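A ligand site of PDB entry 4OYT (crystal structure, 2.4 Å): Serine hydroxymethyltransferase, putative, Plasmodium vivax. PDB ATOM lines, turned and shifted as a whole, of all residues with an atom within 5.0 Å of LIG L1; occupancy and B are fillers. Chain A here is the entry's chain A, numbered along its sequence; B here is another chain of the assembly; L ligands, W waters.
N2 of LIG L1 sits at hydrogen-bond distance from O of Gly 128, at 3.1 Å.
An oxygen (O1) of LIG L1 is in hydrogen-bond range of the backbone NH (N) of Leu 130.
ND1 of His 129 sits at hydrogen-bond distance from O1 of LIG L1 (3.2 Å).
A nitrogen (N2) of LIG L1 sits at hydrogen-bond distance from the backbone carbonyl oxygen (O) of Leu 124.
The side-chain carboxylate (OE1) of Glu 56 of chain B is in hydrogen-bond range of an oxygen (O3) of LG2 L2, 2.6 Å away.
OG1 of Thr 183 lies within hydrogen-bond range of O2 of LG2 L2, 3.0 Å away.
O8 of LG2 L2 lies within hydrogen-bond range of OH of Tyr 64 of chain B, at 2.7 Å.
The backbone carbonyl oxygen (O) of Glu 56 of chain B lies within hydrogen-bond range of the backbone NH (N) of Tyr 63 of chain B.
The side-chain carboxylate of Glu 56 of chain B lies within hydrogen-bond range of the side-chain hydroxyl of Tyr 64 of chain B (2.9 Å).
A ring nitrogen (ND1) of His 129 sits close to the side-chain hydroxyl (OG1) of Thr 183, at 3.5 Å.
N of Thr 183 sits at hydrogen-bond distance from O of Gly 127, 2.7 Å away.
The backbone carbonyl oxygen (O) of Gly 127 lies within hydrogen-bond range of the backbone NH (N) of Ser 184 (2.9 Å).
An oxygen (O7) of LIG L1 lies close to the side-chain carboxylate (OE1) of Glu 56 of chain B (2.8 Å).
Residues that only touch LIG L1: Gly 127, Phe 134, Val 141, Thr 183, Cys 364, Tyr 63 of chain B, Tyr 64 of chain B and Pro 267 of chain B.
Hydrophobic or aromatic side chains that line LIG L1: Leu 124, His 129, Leu 130, Phe 134, Val 141, Tyr 63 of chain B, Tyr 64 of chain B and Pro 267 of chain B.
The nearest printed residue that does not touch LIG L1 is Val 365 (4.01 Å).
Water W3 lies within hydrogen-bond range of the backbone carbonyl oxygen (O) of Leu 124, a nitrogen (N2) of LIG L1 and the backbone NH (N) of Gly 127.
Water W1 lies within hydrogen-bond range of ND2 of Asn 354 (3.1 Å) and N1 of LIG L1 (3.2 Å).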
ATOM      1  N   LEU A 124      24.842  21.593   5.057  1.00  0.00           N
ATOM      2  CA  LEU A 124      25.970  21.849   5.945  1.00  0.00           C
ATOM      3  C   LEU A 124      27.277  21.837   5.179  1.00  0.00           C
ATOM      4  O   LEU A 124      28.120  22.708   5.386  1.00  0.00           O
ATOM      5  CB  LEU A 124      26.022  20.817   7.079  1.00  0.00           C
ATOM      6  CG  LEU A 124      27.025  21.098   8.216  1.00  0.00           C
ATOM      7  CD1 LEU A 124      26.508  20.555   9.535  1.00  0.00           C
ATOM      8  CD2 LEU A 124      28.405  20.536   7.916  1.00  0.00           C
ATOM      9  N   GLY A 127      27.805  24.970   3.553  1.00  0.00           N
ATOM     10  CA  GLY A 127      28.041  26.113   4.455  1.00  0.00           C
ATOM     11  C   GLY A 127      26.890  26.548   5.356  1.00  0.00           C
ATOM     12  O   GLY A 127      27.030  27.500   6.113  1.00  0.00           O
ATOM     13  N   GLY A 128      25.747  25.859   5.259  1.00  0.00           N
ATOM     14  CA  GLY A 128      24.639  26.102   6.175  1.00  0.00           C
ATOM     15  C   GLY A 128      24.895  25.466   7.549  1.00  0.00           C
ATOM     16  O   GLY A 128      25.789  24.629   7.692  1.00  0.00           O
ATOM     17  N   HIS A 129      24.112  25.885   8.548  1.00  0.00           N
ATOM     18  CA  HIS A 129      24.225  25.396   9.916  1.00  0.00           C
ATOM     19  C   HIS A 129      23.347  24.206  10.132  1.00  0.00           C
ATOM     20  O   HIS A 129      22.391  23.976   9.357  1.00  0.00           O
ATOM     21  CB  HIS A 129      23.856  26.496  10.914  1.00  0.00           C
ATOM     22  CG  HIS A 129      24.040  26.088  12.356  1.00  0.00           C
ATOM     23  ND1 HIS A 129      25.257  25.961  12.930  1.00  0.00           N
ATOM     24  CD2 HIS A 129      23.106  25.781  13.340  1.00  0.00           C
ATOM     25  CE1 HIS A 129      25.099  25.565  14.205  1.00  0.00           C
ATOM     26  NE2 HIS A 129      23.786  25.460  14.455  1.00  0.00           N
ATOM     27  N   LEU A 130      23.664  23.428  11.158  1.00  0.00           N
ATOM     28  CA  LEU A 130      22.846  22.272  11.569  1.00  0.00           C
ATOM     29  C   LEU A 130      21.352  22.589  11.678  1.00  0.00           C
ATOM     30  O   LEU A 130      20.521  21.839  11.164  1.00  0.00           O
ATOM     31  CB  LEU A 130      23.328  21.727  12.907  1.00  0.00           C
ATOM     32  CG  LEU A 130      24.646  20.972  12.856  1.00  0.00           C
ATOM     33  CD1 LEU A 130      25.221  20.878  14.264  1.00  0.00           C
ATOM     34  CD2 LEU A 130      24.404  19.592  12.261  1.00  0.00           C
ATOM     35  N   PHE A 134      19.391  20.233   8.720  1.00  0.00           N
ATOM     36  CA  PHE A 134      20.370  19.238   8.307  1.00  0.00           C
ATOM     37  C   PHE A 134      20.018  17.782   8.610  1.00  0.00           C
ATOM     38  O   PHE A 134      19.596  17.439   9.718  1.00  0.00           O
ATOM     39  CB  PHE A 134      21.783  19.562   8.826  1.00  0.00           C
ATOM     40  CG  PHE A 134      22.829  18.610   8.306  1.00  0.00           C
ATOM     41  CD1 PHE A 134      23.157  18.584   6.954  1.00  0.00           C
ATOM     42  CD2 PHE A 134      23.437  17.680   9.159  1.00  0.00           C
ATOM     43  CE1 PHE A 134      24.101  17.683   6.456  1.00  0.00           C
ATOM     44  CE2 PHE A 134      24.371  16.791   8.667  1.00  0.00           C
ATOM     45  CZ  PHE A 134      24.707  16.798   7.314  1.00  0.00           C
ATOM     46  N   ASP A 136      21.247  13.530   6.825  1.00  0.00           N
ATOM     47  CA  ASP A 136      21.924  12.777   5.789  1.00  0.00           C
ATOM     48  C   ASP A 136      21.136  11.527   5.454  1.00  0.00           C
ATOM     49  O   ASP A 136      19.976  11.393   5.858  1.00  0.00           O
ATOM     50  CB  ASP A 136      23.375  12.471   6.169  1.00  0.00           C
ATOM     51  CG  ASP A 136      23.487  11.624   7.435  1.00  0.00           C
ATOM     52  OD1 ASP A 136      22.524  10.891   7.756  1.00  0.00           O
ATOM     53  OD2 ASP A 136      24.550  11.692   8.089  1.00  0.00           O
ATOM     54  N   LYS A 139      20.365   9.357   8.939  1.00  0.00           N
ATOM     55  CA  LYS A 139      19.770   9.962  10.123  1.00  0.00           C
ATOM     56  C   LYS A 139      19.241  11.387   9.943  1.00  0.00           C
ATOM     57  O   LYS A 139      19.812  12.186   9.205  1.00  0.00           O
ATOM     58  CB  LYS A 139      20.810   9.956  11.257  1.00  0.00           C
ATOM     59  CG  LYS A 139      20.224   9.724  12.635  1.00  0.00           C
ATOM     60  CD  LYS A 139      21.284   9.869  13.717  1.00  0.00           C
ATOM     61  CE  LYS A 139      20.647   9.836  15.100  1.00  0.00           C
ATOM     62  NZ  LYS A 139      19.672  10.937  15.334  1.00  0.00           N
ATOM     63  N   VAL A 141      19.690  14.286  11.524  1.00  0.00           N
ATOM     64  CA  VAL A 141      20.792  14.645  12.409  1.00  0.00           C
ATOM     65  C   VAL A 141      20.440  15.827  13.331  1.00  0.00           C
ATOM     66  O   VAL A 141      20.805  15.849  14.508  1.00  0.00           O
ATOM     67  CB  VAL A 141      22.034  14.993  11.550  1.00  0.00           C
ATOM     68  CG1 VAL A 141      23.239  15.374  12.400  1.00  0.00           C
ATOM     69  CG2 VAL A 141      22.356  13.851  10.587  1.00  0.00           C
ATOM     70  N   THR A 183      26.983  29.416   7.953  1.00  0.00           N
ATOM     71  CA  THR A 183      28.038  29.103   8.903  1.00  0.00           C
ATOM     72  C   THR A 183      29.411  29.240   8.243  1.00  0.00           C
ATOM     73  O   THR A 183      30.345  29.754   8.846  1.00  0.00           O
ATOM     74  CB  THR A 183      27.865  27.686   9.450  1.00  0.00           C
ATOM     75  OG1 THR A 183      26.680  27.657  10.260  1.00  0.00           O
ATOM     76  CG2 THR A 183      29.058  27.244  10.283  1.00  0.00           C
ATOM     77  N   SER A 184      29.526  28.777   7.009  1.00  0.00           N
ATOM     78  CA  SER A 184      30.785  28.853   6.322  1.00  0.00           C
ATOM     79  C   SER A 184      30.602  29.316   4.913  1.00  0.00           C
ATOM     80  O   SER A 184      30.595  28.520   3.989  1.00  0.00           O
ATOM     81  CB  SER A 184      31.515  27.524   6.338  1.00  0.00           C
ATOM     82  OG  SER A 184      32.835  27.766   5.915  1.00  0.00           O
ATOM     83  N   ASN A 354      39.708  25.177  11.519  1.00  0.00           N
ATOM     84  CA  ASN A 354      38.903  23.956  11.436  1.00  0.00           C
ATOM     85  C   ASN A 354      38.750  23.482   9.999  1.00  0.00           C
ATOM     86  O   ASN A 354      38.695  24.291   9.077  1.00  0.00           O
ATOM     87  CB  ASN A 354      37.555  24.100  12.167  1.00  0.00           C
ATOM     88  CG  ASN A 354      36.657  25.190  11.577  1.00  0.00           C
ATOM     89  OD1 ASN A 354      36.762  26.359  11.921  1.00  0.00           O
ATOM     90  ND2 ASN A 354      35.762  24.790  10.661  1.00  0.00           N
ATOM     91  N   CYS A 364      31.275  15.177   4.751  1.00  0.00           N
ATOM     92  CA  CYS A 364      31.857  15.890   5.886  1.00  0.00           C
ATOM     93  C   CYS A 364      33.201  15.306   6.397  1.00  0.00           C
ATOM     94  O   CYS A 364      34.044  16.052   6.908  1.00  0.00           O
ATOM     95  CB  CYS A 364      30.830  15.967   7.021  1.00  0.00           C
ATOM     96  SG  CYS A 364      31.484  16.267   8.678  1.00  0.00           S
ATOM     97  N   VAL A 365      33.387  13.995   6.277  1.00  0.00           N
ATOM     98  CA  VAL A 365      34.563  13.309   6.827  1.00  0.00           C
ATOM     99  C   VAL A 365      35.753  13.364   5.864  1.00  0.00           C
ATOM    100  O   VAL A 365      35.638  12.954   4.710  1.00  0.00           O
ATOM    101  CB  VAL A 365      34.265  11.831   7.191  1.00  0.00           C
ATOM    102  CG1 VAL A 365      35.333  11.284   8.141  1.00  0.00           C
ATOM    103  CG2 VAL A 365      32.877  11.685   7.802  1.00  0.00           C
ATOM    104  N   GLU B  56      32.036  22.244  20.366  1.00  0.00           N
ATOM    105  CA  GLU B  56      31.037  21.301  19.865  1.00  0.00           C
ATOM    106  C   GLU B  56      31.551  19.871  19.763  1.00  0.00           C
ATOM    107  O   GLU B  56      32.631  19.612  19.220  1.00  0.00           O
ATOM    108  CB  GLU B  56      30.452  21.769  18.529  1.00  0.00           C
ATOM    109  CG  GLU B  56      31.451  22.388  17.562  1.00  0.00           C
ATOM    110  CD  GLU B  56      30.782  23.374  16.626  1.00  0.00           C
ATOM    111  OE1 GLU B  56      29.536  23.501  16.723  1.00  0.00           O
ATOM    112  OE2 GLU B  56      31.494  24.018  15.805  1.00  0.00           O
ATOM    113  N   TYR B  63      35.007  18.394  17.444  1.00  0.00           N
ATOM    114  CA  TYR B  63      35.159  18.791  16.029  1.00  0.00           C
ATOM    115  C   TYR B  63      36.402  19.635  15.799  1.00  0.00           C
ATOM    116  O   TYR B  63      37.130  19.409  14.826  1.00  0.00           O
ATOM    117  CB  TYR B  63      33.910  19.481  15.452  1.00  0.00           C
ATOM    118  CG  TYR B  63      32.933  18.488  14.885  1.00  0.00           C
ATOM    119  CD1 TYR B  63      33.057  18.036  13.561  1.00  0.00           C
ATOM    120  CD2 TYR B  63      31.920  17.955  15.681  1.00  0.00           C
ATOM    121  CE1 TYR B  63      32.168  17.089  13.051  1.00  0.00           C
ATOM    122  CE2 TYR B  63      31.042  17.013  15.180  1.00  0.00           C
ATOM    123  CZ  TYR B  63      31.165  16.583  13.858  1.00  0.00           C
ATOM    124  OH  TYR B  63      30.288  15.637  13.394  1.00  0.00           O
ATOM    125  N   TYR B  64      36.655  20.589  16.699  1.00  0.00           N
ATOM    126  CA  TYR B  64      37.837  21.448  16.626  1.00  0.00           C
ATOM    127  C   TYR B  64      38.888  20.973  17.612  1.00  0.00           C
ATOM    128  O   TYR B  64      38.592  20.183  18.497  1.00  0.00           O
ATOM    129  CB  TYR B  64      37.483  22.901  16.944  1.00  0.00           C
ATOM    130  CG  TYR B  64      36.347  23.488  16.124  1.00  0.00           C
ATOM    131  CD1 TYR B  64      35.913  22.864  14.946  1.00  0.00           C
ATOM    132  CD2 TYR B  64      35.736  24.679  16.506  1.00  0.00           C
ATOM    133  CE1 TYR B  64      34.894  23.404  14.190  1.00  0.00           C
ATOM    134  CE2 TYR B  64      34.720  25.228  15.753  1.00  0.00           C
ATOM    135  CZ  TYR B  64      34.300  24.579  14.594  1.00  0.00           C
ATOM    136  OH  TYR B  64      33.278  25.111  13.834  1.00  0.00           O
ATOM    137  N   PHE B 266      23.641  17.186  21.584  1.00  0.00           N
ATOM    138  CA  PHE B 266      24.357  17.615  20.389  1.00  0.00           C
ATOM    139  C   PHE B 266      24.531  16.422  19.461  1.00  0.00           C
ATOM    140  O   PHE B 266      25.049  15.407  19.879  1.00  0.00           O
ATOM    141  CB  PHE B 266      25.733  18.119  20.784  1.00  0.00           C
ATOM    142  CG  PHE B 266      26.575  18.530  19.602  1.00  0.00           C
ATOM    143  CD1 PHE B 266      26.303  19.713  18.914  1.00  0.00           C
ATOM    144  CD2 PHE B 266      27.664  17.742  19.199  1.00  0.00           C
ATOM    145  CE1 PHE B 266      27.097  20.102  17.830  1.00  0.00           C
ATOM    146  CE2 PHE B 266      28.453  18.130  18.123  1.00  0.00           C
ATOM    147  CZ  PHE B 266      28.167  19.316  17.438  1.00  0.00           C
ATOM    148  N   PRO B 267      24.181  16.567  18.172  1.00  0.00           N
ATOM    149  CA  PRO B 267      23.818  17.751  17.395  1.00  0.00           C
ATOM    150  C   PRO B 267      22.328  17.911  17.101  1.00  0.00           C
ATOM    151  O   PRO B 267      21.947  18.753  16.286  1.00  0.00           O
ATOM    152  CB  PRO B 267      24.566  17.528  16.090  1.00  0.00           C
ATOM    153  CG  PRO B 267      24.452  16.041  15.891  1.00  0.00           C
ATOM    154  CD  PRO B 267      24.449  15.420  17.268  1.00  0.00           C
HETATM  155  N1  LIG L   1      30.187  24.044   9.507  1.00  0.00           N
HETATM  156  C1  LIG L   1      28.975  24.290   9.003  1.00  0.00           C
HETATM  157  N2  LIG L   1      28.890  24.781   7.742  1.00  0.00           N
HETATM  158  N3  LIG L   1      27.824  24.100   9.702  1.00  0.00           N
HETATM  159  C2  LIG L   1      27.802  23.621  10.975  1.00  0.00           C
HETATM  160  O1  LIG L   1      26.716  23.438  11.598  1.00  0.00           O
HETATM  161  C3  LIG L   1      29.122  23.357  11.566  1.00  0.00           C
HETATM  162  N4  LIG L   1      29.386  22.817  12.811  1.00  0.00           N
HETATM  163  C4  LIG L   1      30.381  21.746  12.596  1.00  0.00           C
HETATM  164  C5  LIG L   1      31.713  22.478  12.475  1.00  0.00           C
HETATM  165  N5  LIG L   1      31.565  23.319  11.282  1.00  0.00           N
HETATM  166  C6  LIG L   1      30.331  23.577  10.740  1.00  0.00           C
HETATM  167  C7  LIG L   1      30.268  20.606  13.585  1.00  0.00           C
HETATM  168  N6  LIG L   1      28.954  20.077  13.278  1.00  0.00           N
HETATM  169  C8  LIG L   1      27.847  16.445  11.654  1.00  0.00           C
HETATM  170  C9  LIG L   1      28.791  17.233  10.969  1.00  0.00           C
HETATM  171  C10 LIG L   1      29.190  18.463  11.482  1.00  0.00           C
HETATM  172  C11 LIG L   1      28.655  18.895  12.696  1.00  0.00           C
HETATM  173  C12 LIG L   1      27.716  18.115  13.361  1.00  0.00           C
HETATM  174  C13 LIG L   1      27.317  16.885  12.848  1.00  0.00           C
HETATM  175  C14 LIG L   1      27.376  15.118  11.139  1.00  0.00           C
HETATM  176  O2  LIG L   1      27.573  14.813   9.974  1.00  0.00           O
HETATM  177  N7  LIG L   1      26.737  14.323  12.014  1.00  0.00           N
HETATM  178  C15 LIG L   1      26.659  12.868  11.981  1.00  0.00           C
HETATM  179  C16 LIG L   1      28.037  12.225  12.076  1.00  0.00           C
HETATM  180  C17 LIG L   1      28.154  11.000  11.165  1.00  0.00           C
HETATM  181  C18 LIG L   1      29.601  10.785  10.741  1.00  0.00           C
HETATM  182  O3  LIG L   1      30.508  11.403  11.364  1.00  0.00           O
HETATM  183  O4  LIG L   1      29.825  10.007   9.787  1.00  0.00           O
HETATM  184  C19 LIG L   1      25.813  12.354  13.109  1.00  0.00           C
HETATM  185  O5  LIG L   1      25.791  13.005  14.189  1.00  0.00           O
HETATM  186  O6  LIG L   1      25.150  11.298  12.941  1.00  0.00           O
HETATM  187  C20 LIG L   1      28.880  23.256  13.899  1.00  0.00           C
HETATM  188  O7  LIG L   1      28.041  22.656  14.562  1.00  0.00           O
HETATM  189  C1  LG2 L   2      30.720  27.848  13.911  1.00  0.00           C
HETATM  190  N1  LG2 L   2      28.185  27.622  14.140  1.00  0.00           N
HETATM  191  O1  LG2 L   2      30.619  28.687  12.985  1.00  0.00           O
HETATM  192  P1  LG2 L   2      25.262  28.171  19.049  1.00  0.00           P
HETATM  193  N2  LG2 L   2      23.736  29.696  13.394  1.00  0.00           N
HETATM  194  C2  LG2 L   2      24.786  29.899  12.700  1.00  0.00           C
HETATM  195  C3  LG2 L   2      26.033  29.505  13.170  1.00  0.00           C
HETATM  196  O2  LG2 L   2      27.090  29.747  12.375  1.00  0.00           O
HETATM  197  C4  LG2 L   2      26.175  28.873  14.389  1.00  0.00           C
HETATM  198  C5  LG2 L   2      24.995  28.697  15.107  1.00  0.00           C
HETATM  199  C6  LG2 L   2      23.801  29.137  14.532  1.00  0.00           C
HETATM  200  C7  LG2 L   2      29.520  26.999  14.281  1.00  0.00           C
HETATM  201  C8  LG2 L   2      29.642  26.518  15.706  1.00  0.00           C
HETATM  202  O3  LG2 L   2      28.465  25.845  16.131  1.00  0.00           O
HETATM  203  O4  LG2 L   2      25.225  29.412  19.932  1.00  0.00           O
HETATM  204  C9  LG2 L   2      24.690  30.580  11.348  1.00  0.00           C
HETATM  205  O5  LG2 L   2      24.056  27.272  19.185  1.00  0.00           O
HETATM  206  O6  LG2 L   2      26.582  27.449  19.029  1.00  0.00           O
HETATM  207  C10 LG2 L   2      27.543  28.443  14.866  1.00  0.00           C
HETATM  208  O7  LG2 L   2      25.199  28.831  17.581  1.00  0.00           O
HETATM  209  C11 LG2 L   2      24.913  28.004  16.454  1.00  0.00           C
HETATM  210  O8  LG2 L   2      31.859  27.416  14.237  1.00  0.00           O
HETATM  211  O   HOH W   1      33.132  25.253   9.157  1.00  0.00           O
HETATM  212  O   HOH W   2      34.532  21.029  11.277  1.00  0.00           O
HETATM  213  O   HOH W   3      30.283  23.741   5.196  1.00  0.00           O
